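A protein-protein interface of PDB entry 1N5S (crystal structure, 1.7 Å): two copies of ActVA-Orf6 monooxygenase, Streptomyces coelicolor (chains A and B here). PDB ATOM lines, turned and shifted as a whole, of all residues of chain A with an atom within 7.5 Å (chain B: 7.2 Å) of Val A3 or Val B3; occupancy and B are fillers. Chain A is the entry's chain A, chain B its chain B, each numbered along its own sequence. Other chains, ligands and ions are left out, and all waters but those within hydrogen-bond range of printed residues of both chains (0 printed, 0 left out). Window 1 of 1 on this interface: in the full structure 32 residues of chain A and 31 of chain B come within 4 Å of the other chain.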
ATOM      1  N   ALA A   1     -21.197  -5.330  -4.004  1.00  0.00           N
ATOM      2  CA  ALA A   1     -20.364  -4.107  -3.843  1.00  0.00           C
ATOM      3  C   ALA A   1     -19.822  -3.958  -2.441  1.00  0.00           C
ATOM      4  O   ALA A   1     -20.425  -4.483  -1.509  1.00  0.00           O
ATOM      5  CB  ALA A   1     -21.212  -2.889  -4.185  1.00  0.00           C
ATOM      6  N   GLU A   2     -18.735  -3.210  -2.263  1.00  0.00           N
ATOM      7  CA  GLU A   2     -18.246  -2.962  -0.888  1.00  0.00           C
ATOM      8  C   GLU A   2     -19.439  -2.580  -0.029  1.00  0.00           C
ATOM      9  O   GLU A   2     -20.392  -1.958  -0.504  1.00  0.00           O
ATOM     10  CB  GLU A   2     -17.227  -1.838  -0.977  1.00  0.00           C
ATOM     11  CG  GLU A   2     -16.863  -1.146   0.335  1.00  0.00           C
ATOM     12  CD  GLU A   2     -16.049  -2.100   1.191  1.00  0.00           C
ATOM     13  OE1 GLU A   2     -14.896  -2.389   0.820  1.00  0.00           O
ATOM     14  OE2 GLU A   2     -16.556  -2.584   2.189  1.00  0.00           O
ATOM     15  N   VAL A   3     -19.476  -2.937   1.272  1.00  0.00           N
ATOM     16  CA  VAL A   3     -20.695  -2.684   2.037  1.00  0.00           C
ATOM     17  C   VAL A   3     -21.033  -1.232   2.283  1.00  0.00           C
ATOM     18  O   VAL A   3     -22.185  -0.848   2.518  1.00  0.00           O
ATOM     19  CB  VAL A   3     -20.656  -3.498   3.372  1.00  0.00           C
ATOM     20  CG1 VAL A   3     -20.941  -4.961   3.049  1.00  0.00           C
ATOM     21  CG2 VAL A   3     -19.340  -3.335   4.105  1.00  0.00           C
ATOM     22  N   ASN A   4     -20.023  -0.372   2.242  1.00  0.00           N
ATOM     23  CA  ASN A   4     -20.205   1.052   2.526  1.00  0.00           C
ATOM     24  C   ASN A   4     -20.083   1.865   1.253  1.00  0.00           C
ATOM     25  O   ASN A   4     -19.812   3.058   1.337  1.00  0.00           O
ATOM     26  CB  ASN A   4     -19.199   1.505   3.594  1.00  0.00           C
ATOM     27  CG  ASN A   4     -17.812   1.736   3.048  1.00  0.00           C
ATOM     28  OD1 ASN A   4     -17.318   0.914   2.279  1.00  0.00           O
ATOM     29  ND2 ASN A   4     -17.178   2.848   3.403  1.00  0.00           N
ATOM     30  N   ASP A   5     -20.219   1.218   0.096  1.00  0.00           N
ATOM     31  CA  ASP A   5     -20.180   2.011  -1.142  1.00  0.00           C
ATOM     32  C   ASP A   5     -21.398   2.919  -1.154  1.00  0.00           C
ATOM     33  O   ASP A   5     -22.532   2.462  -1.040  1.00  0.00           O
ATOM     34  CB  ASP A   5     -20.188   1.042  -2.331  1.00  0.00           C
ATOM     35  CG  ASP A   5     -20.267   1.650  -3.706  1.00  0.00           C
ATOM     36  OD1 ASP A   5     -20.460   2.882  -3.814  1.00  0.00           O
ATOM     37  OD2 ASP A   5     -20.149   0.957  -4.738  1.00  0.00           O
ATOM     38  N   PRO A   6     -21.220   4.219  -1.420  1.00  0.00           N
ATOM     39  CA  PRO A   6     -22.280   5.185  -1.619  1.00  0.00           C
ATOM     40  C   PRO A   6     -23.292   4.881  -2.704  1.00  0.00           C
ATOM     41  O   PRO A   6     -24.434   5.340  -2.602  1.00  0.00           O
ATOM     42  CB  PRO A   6     -21.507   6.441  -2.063  1.00  0.00           C
ATOM     43  CG  PRO A   6     -20.205   6.323  -1.358  1.00  0.00           C
ATOM     44  CD  PRO A   6     -19.880   4.842  -1.589  1.00  0.00           C
ATOM     45  N   VAL A   8     -24.786   2.196  -2.956  1.00  0.00           N
ATOM     46  CA  VAL A   8     -25.841   1.378  -2.354  1.00  0.00           C
ATOM     47  C   VAL A   8     -26.904   2.249  -1.680  1.00  0.00           C
ATOM     48  O   VAL A   8     -26.678   2.705  -0.566  1.00  0.00           O
ATOM     49  CB  VAL A   8     -25.277   0.404  -1.322  1.00  0.00           C
ATOM     50  CG1 VAL A   8     -26.447  -0.337  -0.677  1.00  0.00           C
ATOM     51  CG2 VAL A   8     -24.283  -0.545  -2.003  1.00  0.00           C
ATOM     52  N   VAL A  11     -31.484  -1.502   0.658  1.00  0.00           N
ATOM     53  CA  VAL A  11     -31.090  -2.922   0.969  1.00  0.00           C
ATOM     54  C   VAL A  11     -32.349  -3.657   1.393  1.00  0.00           C
ATOM     55  O   VAL A  11     -33.228  -3.123   2.105  1.00  0.00           O
ATOM     56  CB  VAL A  11     -30.090  -2.892   2.123  1.00  0.00           C
ATOM     57  CG1 VAL A  11     -29.961  -4.251   2.862  1.00  0.00           C
ATOM     58  CG2 VAL A  11     -28.700  -2.376   1.778  1.00  0.00           C
ATOM     59  N   LEU A  46     -27.117  -4.791  -7.391  1.00  0.00           N
ATOM     60  CA  LEU A  46     -25.729  -4.747  -6.993  1.00  0.00           C
ATOM     61  C   LEU A  46     -25.254  -6.090  -6.389  1.00  0.00           C
ATOM     62  O   LEU A  46     -24.122  -6.504  -6.690  1.00  0.00           O
ATOM     63  CB  LEU A  46     -25.392  -3.637  -5.977  1.00  0.00           C
ATOM     64  CG  LEU A  46     -25.623  -2.184  -6.532  1.00  0.00           C
ATOM     65  CD1 LEU A  46     -25.420  -1.128  -5.441  1.00  0.00           C
ATOM     66  CD2 LEU A  46     -24.674  -1.982  -7.678  1.00  0.00           C
ATOM     67  N   SER A  47     -26.128  -6.766  -5.646  1.00  0.00           N
ATOM     68  CA  SER A  47     -25.702  -8.072  -5.113  1.00  0.00           C
ATOM     69  C   SER A  47     -26.768  -8.734  -4.243  1.00  0.00           C
ATOM     70  O   SER A  47     -27.755  -8.112  -3.839  1.00  0.00           O
ATOM     71  CB  SER A  47     -24.425  -7.945  -4.229  1.00  0.00           C
ATOM     72  OG  SER A  47     -24.840  -7.406  -2.963  1.00  0.00           O
ATOM     73  N   ALA A  48     -26.636 -10.067  -4.190  1.00  0.00           N
ATOM     74  CA  ALA A  48     -27.562 -10.819  -3.294  1.00  0.00           C
ATOM     75  C   ALA A  48     -26.642 -11.832  -2.568  1.00  0.00           C
ATOM     76  O   ALA A  48     -26.107 -12.659  -3.330  1.00  0.00           O
ATOM     77  CB  ALA A  48     -28.751 -11.428  -3.929  1.00  0.00           C
ATOM     78  N   THR A  49     -26.471 -11.726  -1.242  1.00  0.00           N
ATOM     79  CA  THR A  49     -25.557 -12.670  -0.580  1.00  0.00           C
ATOM     80  C   THR A  49     -26.371 -13.570   0.326  1.00  0.00           C
ATOM     81  O   THR A  49     -27.069 -13.065   1.206  1.00  0.00           O
ATOM     82  CB  THR A  49     -24.440 -11.996   0.232  1.00  0.00           C
ATOM     83  OG1 THR A  49     -23.572 -11.262  -0.680  1.00  0.00           O
ATOM     84  CG2 THR A  49     -23.584 -13.030   0.959  1.00  0.00           C
ATOM     85  N   HIS A  51     -26.711 -16.452   3.264  1.00  0.00           N
ATOM     86  CA  HIS A  51     -25.942 -16.966   4.381  1.00  0.00           C
ATOM     87  C   HIS A  51     -26.717 -18.093   5.037  1.00  0.00           C
ATOM     88  O   HIS A  51     -27.951 -18.025   5.110  1.00  0.00           O
ATOM     89  CB  HIS A  51     -25.812 -15.816   5.433  1.00  0.00           C
ATOM     90  CG  HIS A  51     -25.249 -14.522   4.987  1.00  0.00           C
ATOM     91  ND1 HIS A  51     -26.023 -13.664   4.175  1.00  0.00           N
ATOM     92  CD2 HIS A  51     -24.117 -13.859   5.211  1.00  0.00           C
ATOM     93  CE1 HIS A  51     -25.328 -12.578   3.904  1.00  0.00           C
ATOM     94  NE2 HIS A  51     -24.141 -12.651   4.546  1.00  0.00           N
ATOM     95  N   TYR A  62     -28.798 -10.941   2.130  1.00  0.00           N
ATOM     96  CA  TYR A  62     -28.528  -9.488   2.264  1.00  0.00           C
ATOM     97  C   TYR A  62     -28.328  -9.021   0.812  1.00  0.00           C
ATOM     98  O   TYR A  62     -27.395  -9.454   0.114  1.00  0.00           O
ATOM     99  CB  TYR A  62     -27.272  -9.258   3.087  1.00  0.00           C
ATOM    100  CG  TYR A  62     -26.847  -7.805   3.180  1.00  0.00           C
ATOM    101  CD1 TYR A  62     -27.459  -7.024   4.152  1.00  0.00           C
ATOM    102  CD2 TYR A  62     -25.854  -7.294   2.353  1.00  0.00           C
ATOM    103  CE1 TYR A  62     -27.060  -5.659   4.273  1.00  0.00           C
ATOM    104  CE2 TYR A  62     -25.465  -5.942   2.465  1.00  0.00           C
ATOM    105  CZ  TYR A  62     -26.103  -5.176   3.406  1.00  0.00           C
ATOM    106  OH  TYR A  62     -25.746  -3.830   3.526  1.00  0.00           O
ATOM    107  N   ALA A  63     -29.261  -8.186   0.325  1.00  0.00           N
ATOM    108  CA  ALA A  63     -29.231  -7.734  -1.071  1.00  0.00           C
ATOM    109  C   ALA A  63     -29.069  -6.230  -1.200  1.00  0.00           C
ATOM    110  O   ALA A  63     -29.772  -5.454  -0.524  1.00  0.00           O
ATOM    111  CB  ALA A  63     -30.600  -8.096  -1.677  1.00  0.00           C
ATOM    112  N   GLN A  64     -28.106  -5.831  -2.010  1.00  0.00           N
ATOM    113  CA  GLN A  64     -27.835  -4.392  -2.221  1.00  0.00           C
ATOM    114  C   GLN A  64     -28.407  -3.937  -3.568  1.00  0.00           C
ATOM    115  O   GLN A  64     -28.335  -4.627  -4.571  1.00  0.00           O
ATOM    116  CB  GLN A  64     -26.325  -4.174  -2.347  1.00  0.00           C
ATOM    117  CG  GLN A  64     -25.540  -4.539  -1.075  1.00  0.00           C
ATOM    118  CD  GLN A  64     -24.046  -4.574  -1.344  1.00  0.00           C
ATOM    119  OE1 GLN A  64     -23.592  -5.161  -2.347  1.00  0.00           O
ATOM    120  NE2 GLN A  64     -23.201  -3.965  -0.496  1.00  0.00           N
ATOM    121  N   PRO A 105     -28.585   2.126   4.035  1.00  0.00           N
ATOM    122  CA  PRO A 105     -27.352   2.247   4.768  1.00  0.00           C
ATOM    123  C   PRO A 105     -27.215   3.668   5.343  1.00  0.00           C
ATOM    124  O   PRO A 105     -27.433   4.654   4.610  1.00  0.00           O
ATOM    125  CB  PRO A 105     -26.246   1.918   3.771  1.00  0.00           C
ATOM    126  CG  PRO A 105     -26.967   1.051   2.763  1.00  0.00           C
ATOM    127  CD  PRO A 105     -28.311   1.761   2.609  1.00  0.00           C
ATOM    128  N   GLY A 107     -24.559   4.507   8.048  1.00  0.00           N
ATOM    129  CA  GLY A 107     -23.265   4.752   8.663  1.00  0.00           C
ATOM    130  C   GLY A 107     -22.493   3.434   8.639  1.00  0.00           C
ATOM    131  O   GLY A 107     -23.105   2.359   8.622  1.00  0.00           O
ATOM    132  N   ALA A 108     -21.174   3.576   8.681  1.00  0.00           N
ATOM    133  CA  ALA A 108     -20.342   2.381   8.661  1.00  0.00           C
ATOM    134  C   ALA A 108     -19.048   2.602   9.405  1.00  0.00           C
ATOM    135  O   ALA A 108     -18.588   3.685   9.841  1.00  0.00           O
ATOM    136  CB  ALA A 108     -20.115   1.861   7.254  1.00  0.00           C
ATOM    137  N   ILE A 109     -18.498   1.443   9.716  1.00  0.00           N
ATOM    138  CA  ILE A 109     -17.220   1.372  10.403  1.00  0.00           C
ATOM    139  C   ILE A 109     -16.363   0.436   9.557  1.00  0.00           C
ATOM    140  O   ILE A 109     -16.762  -0.722   9.387  1.00  0.00           O
ATOM    141  CB  ILE A 109     -17.350   0.922  11.853  1.00  0.00           C
ATOM    142  CG1 ILE A 109     -18.296   1.830  12.640  1.00  0.00           C
ATOM    143  CG2 ILE A 109     -15.945   0.912  12.443  1.00  0.00           C
ATOM    144  CD1 ILE A 109     -18.656   1.430  14.053  1.00  0.00           C
ATOM    145  N   LEU A 110     -15.306   1.016   8.973  1.00  0.00           N
ATOM    146  CA  LEU A 110     -14.430   0.118   8.188  1.00  0.00           C
ATOM    147  C   LEU A 110     -13.097  -0.001   8.882  1.00  0.00           C
ATOM    148  O   LEU A 110     -12.800   0.567   9.949  1.00  0.00           O
ATOM    149  CB  LEU A 110     -14.577   0.360   6.684  1.00  0.00           C
ATOM    150  CG  LEU A 110     -15.723  -0.514   6.089  1.00  0.00           C
ATOM    151  CD1 LEU A 110     -17.062   0.209   6.097  1.00  0.00           C
ATOM    152  CD2 LEU A 110     -15.415  -1.105   4.736  1.00  0.00           C
ATOM    153  N   ALA B   1     -15.737  -4.749   3.451  1.00  0.00           N
ATOM    154  CA  ALA B   1     -15.245  -5.696   2.425  1.00  0.00           C
ATOM    155  C   ALA B   1     -16.294  -5.927   1.340  1.00  0.00           C
ATOM    156  O   ALA B   1     -17.495  -5.812   1.625  1.00  0.00           O
ATOM    157  CB  ALA B   1     -14.905  -7.056   3.035  1.00  0.00           C
ATOM    158  N   GLU B   2     -15.828  -6.388   0.176  1.00  0.00           N
ATOM    159  CA  GLU B   2     -16.865  -6.775  -0.818  1.00  0.00           C
ATOM    160  C   GLU B   2     -17.677  -7.859  -0.123  1.00  0.00           C
ATOM    161  O   GLU B   2     -17.102  -8.581   0.743  1.00  0.00           O
ATOM    162  CB  GLU B   2     -16.185  -7.350  -2.063  1.00  0.00           C
ATOM    163  CG  GLU B   2     -16.237  -6.396  -3.255  1.00  0.00           C
ATOM    164  CD  GLU B   2     -17.617  -6.264  -3.863  1.00  0.00           C
ATOM    165  OE1 GLU B   2     -17.786  -5.378  -4.727  1.00  0.00           O
ATOM    166  OE2 GLU B   2     -18.626  -6.974  -3.563  1.00  0.00           O
ATOM    167  N   VAL B   3     -18.939  -7.981  -0.502  1.00  0.00           N
ATOM    168  CA  VAL B   3     -19.822  -8.940   0.149  1.00  0.00           C
ATOM    169  C   VAL B   3     -19.367 -10.375  -0.082  1.00  0.00           C
ATOM    170  O   VAL B   3     -19.664 -11.238   0.792  1.00  0.00           O
ATOM    171  CB  VAL B   3     -21.323  -8.827  -0.235  1.00  0.00           C
ATOM    172  CG1 VAL B   3     -21.894  -7.464   0.163  1.00  0.00           C
ATOM    173  CG2 VAL B   3     -21.517  -9.145  -1.714  1.00  0.00           C
ATOM    174  N   ASN B   4     -18.655 -10.652  -1.179  1.00  0.00           N
ATOM    175  CA  ASN B   4     -18.215 -12.011  -1.424  1.00  0.00           C
ATOM    176  C   ASN B   4     -16.717 -12.207  -1.222  1.00  0.00           C
ATOM    177  O   ASN B   4     -16.155 -13.161  -1.756  1.00  0.00           O
ATOM    178  CB  ASN B   4     -18.641 -12.432  -2.836  1.00  0.00           C
ATOM    179  CG  ASN B   4     -17.895 -11.612  -3.860  1.00  0.00           C
ATOM    180  OD1 ASN B   4     -17.677 -10.412  -3.654  1.00  0.00           O
ATOM    181  ND2 ASN B   4     -17.512 -12.298  -4.953  1.00  0.00           N
ATOM    182  N   ASP B   5     -16.130 -11.286  -0.457  1.00  0.00           N
ATOM    183  CA  ASP B   5     -14.697 -11.401  -0.124  1.00  0.00           C
ATOM    184  C   ASP B   5     -14.514 -12.650   0.694  1.00  0.00           C
ATOM    185  O   ASP B   5     -15.175 -12.826   1.720  1.00  0.00           O
ATOM    186  CB  ASP B   5     -14.340 -10.150   0.665  1.00  0.00           C
ATOM    187  CG  ASP B   5     -12.873  -9.996   0.993  1.00  0.00           C
ATOM    188  OD1 ASP B   5     -12.226 -11.001   1.304  1.00  0.00           O
ATOM    189  OD2 ASP B   5     -12.349  -8.859   1.008  1.00  0.00           O
ATOM    190  N   PRO B   6     -13.634 -13.565   0.311  1.00  0.00           N
ATOM    191  CA  PRO B   6     -13.335 -14.789   0.995  1.00  0.00           C
ATOM    192  C   PRO B   6     -12.760 -14.659   2.409  1.00  0.00           C
ATOM    193  O   PRO B   6     -12.833 -15.645   3.181  1.00  0.00           O
ATOM    194  CB  PRO B   6     -12.292 -15.479   0.073  1.00  0.00           C
ATOM    195  CG  PRO B   6     -11.592 -14.306  -0.552  1.00  0.00           C
ATOM    196  CD  PRO B   6     -12.797 -13.439  -0.939  1.00  0.00           C
ATOM    197  N   VAL B   8     -14.365 -13.014   4.652  1.00  0.00           N
ATOM    198  CA  VAL B   8     -15.490 -12.908   5.606  1.00  0.00           C
ATOM    199  C   VAL B   8     -15.963 -14.304   5.948  1.00  0.00           C
ATOM    200  O   VAL B   8     -16.661 -14.936   5.087  1.00  0.00           O
ATOM    201  CB  VAL B   8     -16.684 -12.196   4.953  1.00  0.00           C
ATOM    202  CG1 VAL B   8     -17.897 -12.075   5.880  1.00  0.00           C
ATOM    203  CG2 VAL B   8     -16.297 -10.834   4.406  1.00  0.00           C
ATOM    204  N   VAL B  11     -20.670 -13.601   9.912  1.00  0.00           N
ATOM    205  CA  VAL B  11     -21.458 -12.378   9.858  1.00  0.00           C
ATOM    206  C   VAL B  11     -22.484 -12.272  10.997  1.00  0.00           C
ATOM    207  O   VAL B  11     -23.038 -13.302  11.370  1.00  0.00           O
ATOM    208  CB  VAL B  11     -22.264 -12.337   8.496  1.00  0.00           C
ATOM    209  CG1 VAL B  11     -23.331 -11.239   8.539  1.00  0.00           C
ATOM    210  CG2 VAL B  11     -21.267 -11.979   7.320  1.00  0.00           C
ATOM    211  N   LEU B  46     -13.915  -6.882  10.039  1.00  0.00           N
ATOM    212  CA  LEU B  46     -13.909  -6.439   8.630  1.00  0.00           C
ATOM    213  C   LEU B  46     -14.844  -5.274   8.387  1.00  0.00           C
ATOM    214  O   LEU B  46     -14.423  -4.374   7.609  1.00  0.00           O
ATOM    215  CB  LEU B  46     -14.255  -7.615   7.704  1.00  0.00           C
ATOM    216  CG  LEU B  46     -13.259  -8.779   7.751  1.00  0.00           C
ATOM    217  CD1 LEU B  46     -13.776  -9.977   6.993  1.00  0.00           C
ATOM    218  CD2 LEU B  46     -11.882  -8.413   7.126  1.00  0.00           C
ATOM    219  N   SER B  47     -16.016  -5.158   8.945  1.00  0.00           N
ATOM    220  CA  SER B  47     -16.883  -3.997   8.672  1.00  0.00           C
ATOM    221  C   SER B  47     -18.121  -4.023   9.547  1.00  0.00           C
ATOM    222  O   SER B  47     -18.474  -5.113  10.011  1.00  0.00           O
ATOM    223  CB  SER B  47     -17.389  -3.901   7.218  1.00  0.00           C
ATOM    224  OG  SER B  47     -18.341  -4.952   7.026  1.00  0.00           O
ATOM    225  N   ALA B  48     -18.728  -2.862   9.775  1.00  0.00           N
ATOM    226  CA  ALA B  48     -20.001  -2.788  10.506  1.00  0.00           C
ATOM    227  C   ALA B  48     -20.807  -1.803   9.661  1.00  0.00           C
ATOM    228  O   ALA B  48     -20.266  -0.696   9.411  1.00  0.00           O
ATOM    229  CB  ALA B  48     -19.937  -2.372  11.953  1.00  0.00           C
ATOM    230  N   THR B  49     -21.950  -2.143   9.120  1.00  0.00           N
ATOM    231  CA  THR B  49     -22.703  -1.212   8.288  1.00  0.00           C
ATOM    232  C   THR B  49     -24.077  -1.083   8.920  1.00  0.00           C
ATOM    233  O   THR B  49     -24.868  -2.022   9.084  1.00  0.00           O
ATOM    234  CB  THR B  49     -22.882  -1.658   6.832  1.00  0.00           C
ATOM    235  OG1 THR B  49     -21.627  -1.833   6.190  1.00  0.00           O
ATOM    236  CG2 THR B  49     -23.739  -0.629   6.096  1.00  0.00           C
ATOM    237  N   HIS B  51     -27.825   0.431   9.196  1.00  0.00           N
ATOM    238  CA  HIS B  51     -28.907   0.820   8.283  1.00  0.00           C
ATOM    239  C   HIS B  51     -30.124   1.288   9.075  1.00  0.00           C
ATOM    240  O   HIS B  51     -30.302   0.856  10.193  1.00  0.00           O
ATOM    241  CB  HIS B  51     -29.474  -0.345   7.424  1.00  0.00           C
ATOM    242  CG  HIS B  51     -28.451  -1.150   6.732  1.00  0.00           C
ATOM    243  ND1 HIS B  51     -27.532  -1.943   7.454  1.00  0.00           N
ATOM    244  CD2 HIS B  51     -28.241  -1.390   5.392  1.00  0.00           C
ATOM    245  CE1 HIS B  51     -26.728  -2.539   6.573  1.00  0.00           C
ATOM    246  NE2 HIS B  51     -27.146  -2.208   5.356  1.00  0.00           N
ATOM    247  N   TYR B  62     -25.240  -4.825   9.770  1.00  0.00           N
ATOM    248  CA  TYR B  62     -24.693  -6.019   9.072  1.00  0.00           C
ATOM    249  C   TYR B  62     -23.202  -5.946   9.341  1.00  0.00           C
ATOM    250  O   TYR B  62     -22.515  -5.026   8.811  1.00  0.00           O
ATOM    251  CB  TYR B  62     -24.988  -5.960   7.582  1.00  0.00           C
ATOM    252  CG  TYR B  62     -24.346  -7.091   6.753  1.00  0.00           C
ATOM    253  CD1 TYR B  62     -23.106  -7.015   6.126  1.00  0.00           C
ATOM    254  CD2 TYR B  62     -25.099  -8.229   6.611  1.00  0.00           C
ATOM    255  CE1 TYR B  62     -22.614  -8.093   5.346  1.00  0.00           C
ATOM    256  CE2 TYR B  62     -24.617  -9.316   5.844  1.00  0.00           C
ATOM    257  CZ  TYR B  62     -23.412  -9.216   5.214  1.00  0.00           C
ATOM    258  OH  TYR B  62     -22.863 -10.245   4.444  1.00  0.00           O
ATOM    259  N   GLN B  64     -19.270  -7.727   9.246  1.00  0.00           N
ATOM    260  CA  GLN B  64     -18.403  -8.767   8.649  1.00  0.00           C
ATOM    261  C   GLN B  64     -17.218  -9.001   9.551  1.00  0.00           C
ATOM    262  O   GLN B  64     -16.567  -8.059  10.041  1.00  0.00           O
ATOM    263  CB  GLN B  64     -17.861  -8.299   7.294  1.00  0.00           C
ATOM    264  CG  GLN B  64     -18.950  -8.059   6.233  1.00  0.00           C
ATOM    265  CD  GLN B  64     -18.294  -7.471   4.988  1.00  0.00           C
ATOM    266  OE1 GLN B  64     -17.514  -6.527   5.103  1.00  0.00           O
ATOM    267  NE2 GLN B  64     -18.517  -8.009   3.783  1.00  0.00           N
ATOM    268  N   PRO B 105     -21.564 -16.683   5.264  1.00  0.00           N
ATOM    269  CA  PRO B 105     -21.814 -16.520   3.828  1.00  0.00           C
ATOM    270  C   PRO B 105     -21.626 -17.881   3.124  1.00  0.00           C
ATOM    271  O   PRO B 105     -20.663 -18.573   3.424  1.00  0.00           O
ATOM    272  CB  PRO B 105     -20.781 -15.538   3.271  1.00  0.00           C
ATOM    273  CG  PRO B 105     -20.165 -14.956   4.518  1.00  0.00           C
ATOM    274  CD  PRO B 105     -20.361 -15.887   5.663  1.00  0.00           C
ATOM    275  N   GLY B 107     -23.110 -18.124  -0.437  1.00  0.00           N
ATOM    276  CA  GLY B 107     -23.186 -18.002  -1.904  1.00  0.00           C
ATOM    277  C   GLY B 107     -23.669 -16.585  -2.226  1.00  0.00           C
ATOM    278  O   GLY B 107     -24.260 -15.840  -1.433  1.00  0.00           O
ATOM    279  N   ALA B 108     -23.271 -16.154  -3.416  1.00  0.00           N
ATOM    280  CA  ALA B 108     -23.632 -14.763  -3.771  1.00  0.00           C
ATOM    281  C   ALA B 108     -23.965 -14.644  -5.230  1.00  0.00           C
ATOM    282  O   ALA B 108     -23.335 -15.271  -6.060  1.00  0.00           O
ATOM    283  CB  ALA B 108     -22.437 -13.819  -3.552  1.00  0.00           C
ATOM    284  N   ILE B 109     -24.917 -13.746  -5.515  1.00  0.00           N
ATOM    285  CA  ILE B 109     -25.267 -13.456  -6.917  1.00  0.00           C
ATOM    286  C   ILE B 109     -24.810 -12.047  -7.196  1.00  0.00           C
ATOM    287  O   ILE B 109     -25.196 -11.099  -6.460  1.00  0.00           O
ATOM    288  CB  ILE B 109     -26.740 -13.599  -7.161  1.00  0.00           C
ATOM    289  CG1 ILE B 109     -27.205 -15.042  -6.884  1.00  0.00           C
ATOM    290  CG2 ILE B 109     -27.091 -13.157  -8.603  1.00  0.00           C
ATOM    291  CD1 ILE B 109     -26.331 -16.104  -7.546  1.00  0.00           C
ATOM    292  N   LEU B 110     -23.860 -11.922  -8.162  1.00  0.00           N
ATOM    293  CA  LEU B 110     -23.306 -10.578  -8.446  1.00  0.00           C
ATOM    294  C   LEU B 110     -23.298 -10.230  -9.922  1.00  0.00           C
ATOM    295  O   LEU B 110     -23.230 -11.148 -10.730  1.00  0.00           O
ATOM    296  CB  LEU B 110     -21.837 -10.528  -8.033  1.00  0.00           C
ATOM    297  CG  LEU B 110     -21.494 -10.835  -6.563  1.00  0.00           C
ATOM    298  CD1 LEU B 110     -20.148 -11.521  -6.503  1.00  0.00           C
ATOM    299  CD2 LEU B 110     -21.583  -9.500  -5.859  1.00  0.00           C
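Ala A1 touches Val B3, and with the chains exchanged Val A3 touches Ala B1.
Ser A47 touches Ile B109, and with the chains exchanged Ile A109 touches Ser B47.
Thr A49 touches Gly B107, and with the chains exchanged Gly A107 touches Thr B49.
His A51 touches Pro B105, and with the chains exchanged Pro A105 touches His B51.
Positions printed for both chains: 1, 2, 3, 4, 5, 6, 8, 11, 46, 47, 48, 49, 51, 62, 64, 105, 107, 108, 109 and 110.
Of the 29 pairs that touch across the chains among the printed residues, 27 have their exchanged pair printed and touching as well.
The backbone carbonyl oxygen (O) of Glu A2 sits at hydrogen-bond distance from the side-chain amide nitrogen (NE2) of Gln A64 (3.5 Å).
The backbone carbonyl oxygen of Thr A49 sits at hydrogen-bond distance from a ring nitrogen (ND1) of His A51 (3.2 Å).
OE1 of Gln B64 lies within hydrogen-bond range of N of Ala B1, at 3.0 Å.
The backbone carbonyl oxygen (O) of Glu B2 is in hydrogen-bond range of the side-chain amide nitrogen (NE2) of Gln B64, 3.4 Å away.
O of Gln B64 sits at hydrogen-bond distance from N of Leu B46 (2.9 Å).
OG of Ser B47 is in hydrogen-bond range of OE1 of Gln B64 (2.6 Å).
N of Ala A1 is in hydrogen-bond range of OE2 of Glu B2 (3.1 Å).
OE2 of Glu A2 lies within hydrogen-bond range of N of Ala B1 (2.6 Å).
The backbone NH of Glu A2 lies within hydrogen-bond range of the side-chain carboxylate of Glu B2 (3.4 Å).
O of Ala A48 is in hydrogen-bond range of N of Ile B109 (2.7 Å).
A ring nitrogen (NE2) of His A51 lies within hydrogen-bond range of the side-chain hydroxyl of Tyr B62 (2.7 Å).
A ring nitrogen (NE2) of His B51 sits at hydrogen-bond distance from the side-chain hydroxyl (OH) of Tyr A62 (2.8 Å).
O of Ala B48 is in hydrogen-bond range of N of Ile A109, 2.8 Å away.
Of the 20 printed residues of chain B, 14 touch a printed residue of chain A.
Hydrophobic or aromatic side chains of chain B that line the printed part of chain A: Val B3, His B51, Tyr B62, Ala B108, Ile B109 and Leu B110.
Of the 21 printed residues of chain A, 15 touch a printed residue of chain B.
Printed residues of chain A that touch a printed residue of chain B: Ala A1, Glu A2, Val A3, Val A11, Ser A47, Ala A48, Thr A49, His A51, Tyr A62, Gln A64, Pro A105, Gly A107, Ala A108, Ile A109 and Leu A110.
Hydrophobic or aromatic side chains of chain A within 4 Å of the printed part of chain B: Val A3, Val A11, His A51, Tyr A62, Pro A105, Ala A108 and Leu A110.
Along chain A the printed residues that touch a printed residue of chain B span positions 1 to 110.
Printed residues of chain B within 4 Å of Val A3: Ala B1 (3.5 Å), Val B3 (3.9 Å), Ser B47 (3.5 Å), Thr B49 (3.4 Å) and Gln B64 (3.8 Å).
Of chain A, only Ala A1 (3.7 Å), Val A3 (3.9 Å), Ser A47 (3.95 Å), Thr A49 (3.1 Å) and Gln A64 (3.8 Å) come within 4 Å of Val B3.
Of the printed residues of chain B, Tyr A62 touches His B51 and Tyr B62.
Printed residues of chain A within 4 Å of Ala B48: Ala A108 and Ile A109.
The nearest residue of chain A that does not touch Val B3 is Tyr A62 (4.5 Å).
The nearest printed residue of chain A that does not touch Ala B1 is Ala A1 (4.5 Å).
Val A3 touches Ala B1.
Val B3 touches Val A3.
Val A3 touches Ser B47 (CG2 to OG, 3.5 Å).
His B51 touches Val A11.
OG of Ser A47 touches CG2 of Val B3, at 3.95 Å.
Ile B109 touches Ser A47 (O to CA, 3.4 Å).
Ser A47 touches Leu B110 (CB to CD2, 3.6 Å).
Ala A48 touches Ala B108 (O to CA, 3.3 Å).
Pro B105 touches His A51 (CA to CD2, 3.8 Å).
Ile A109 touches Ser B47 (O to CA, 3.4 Å).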
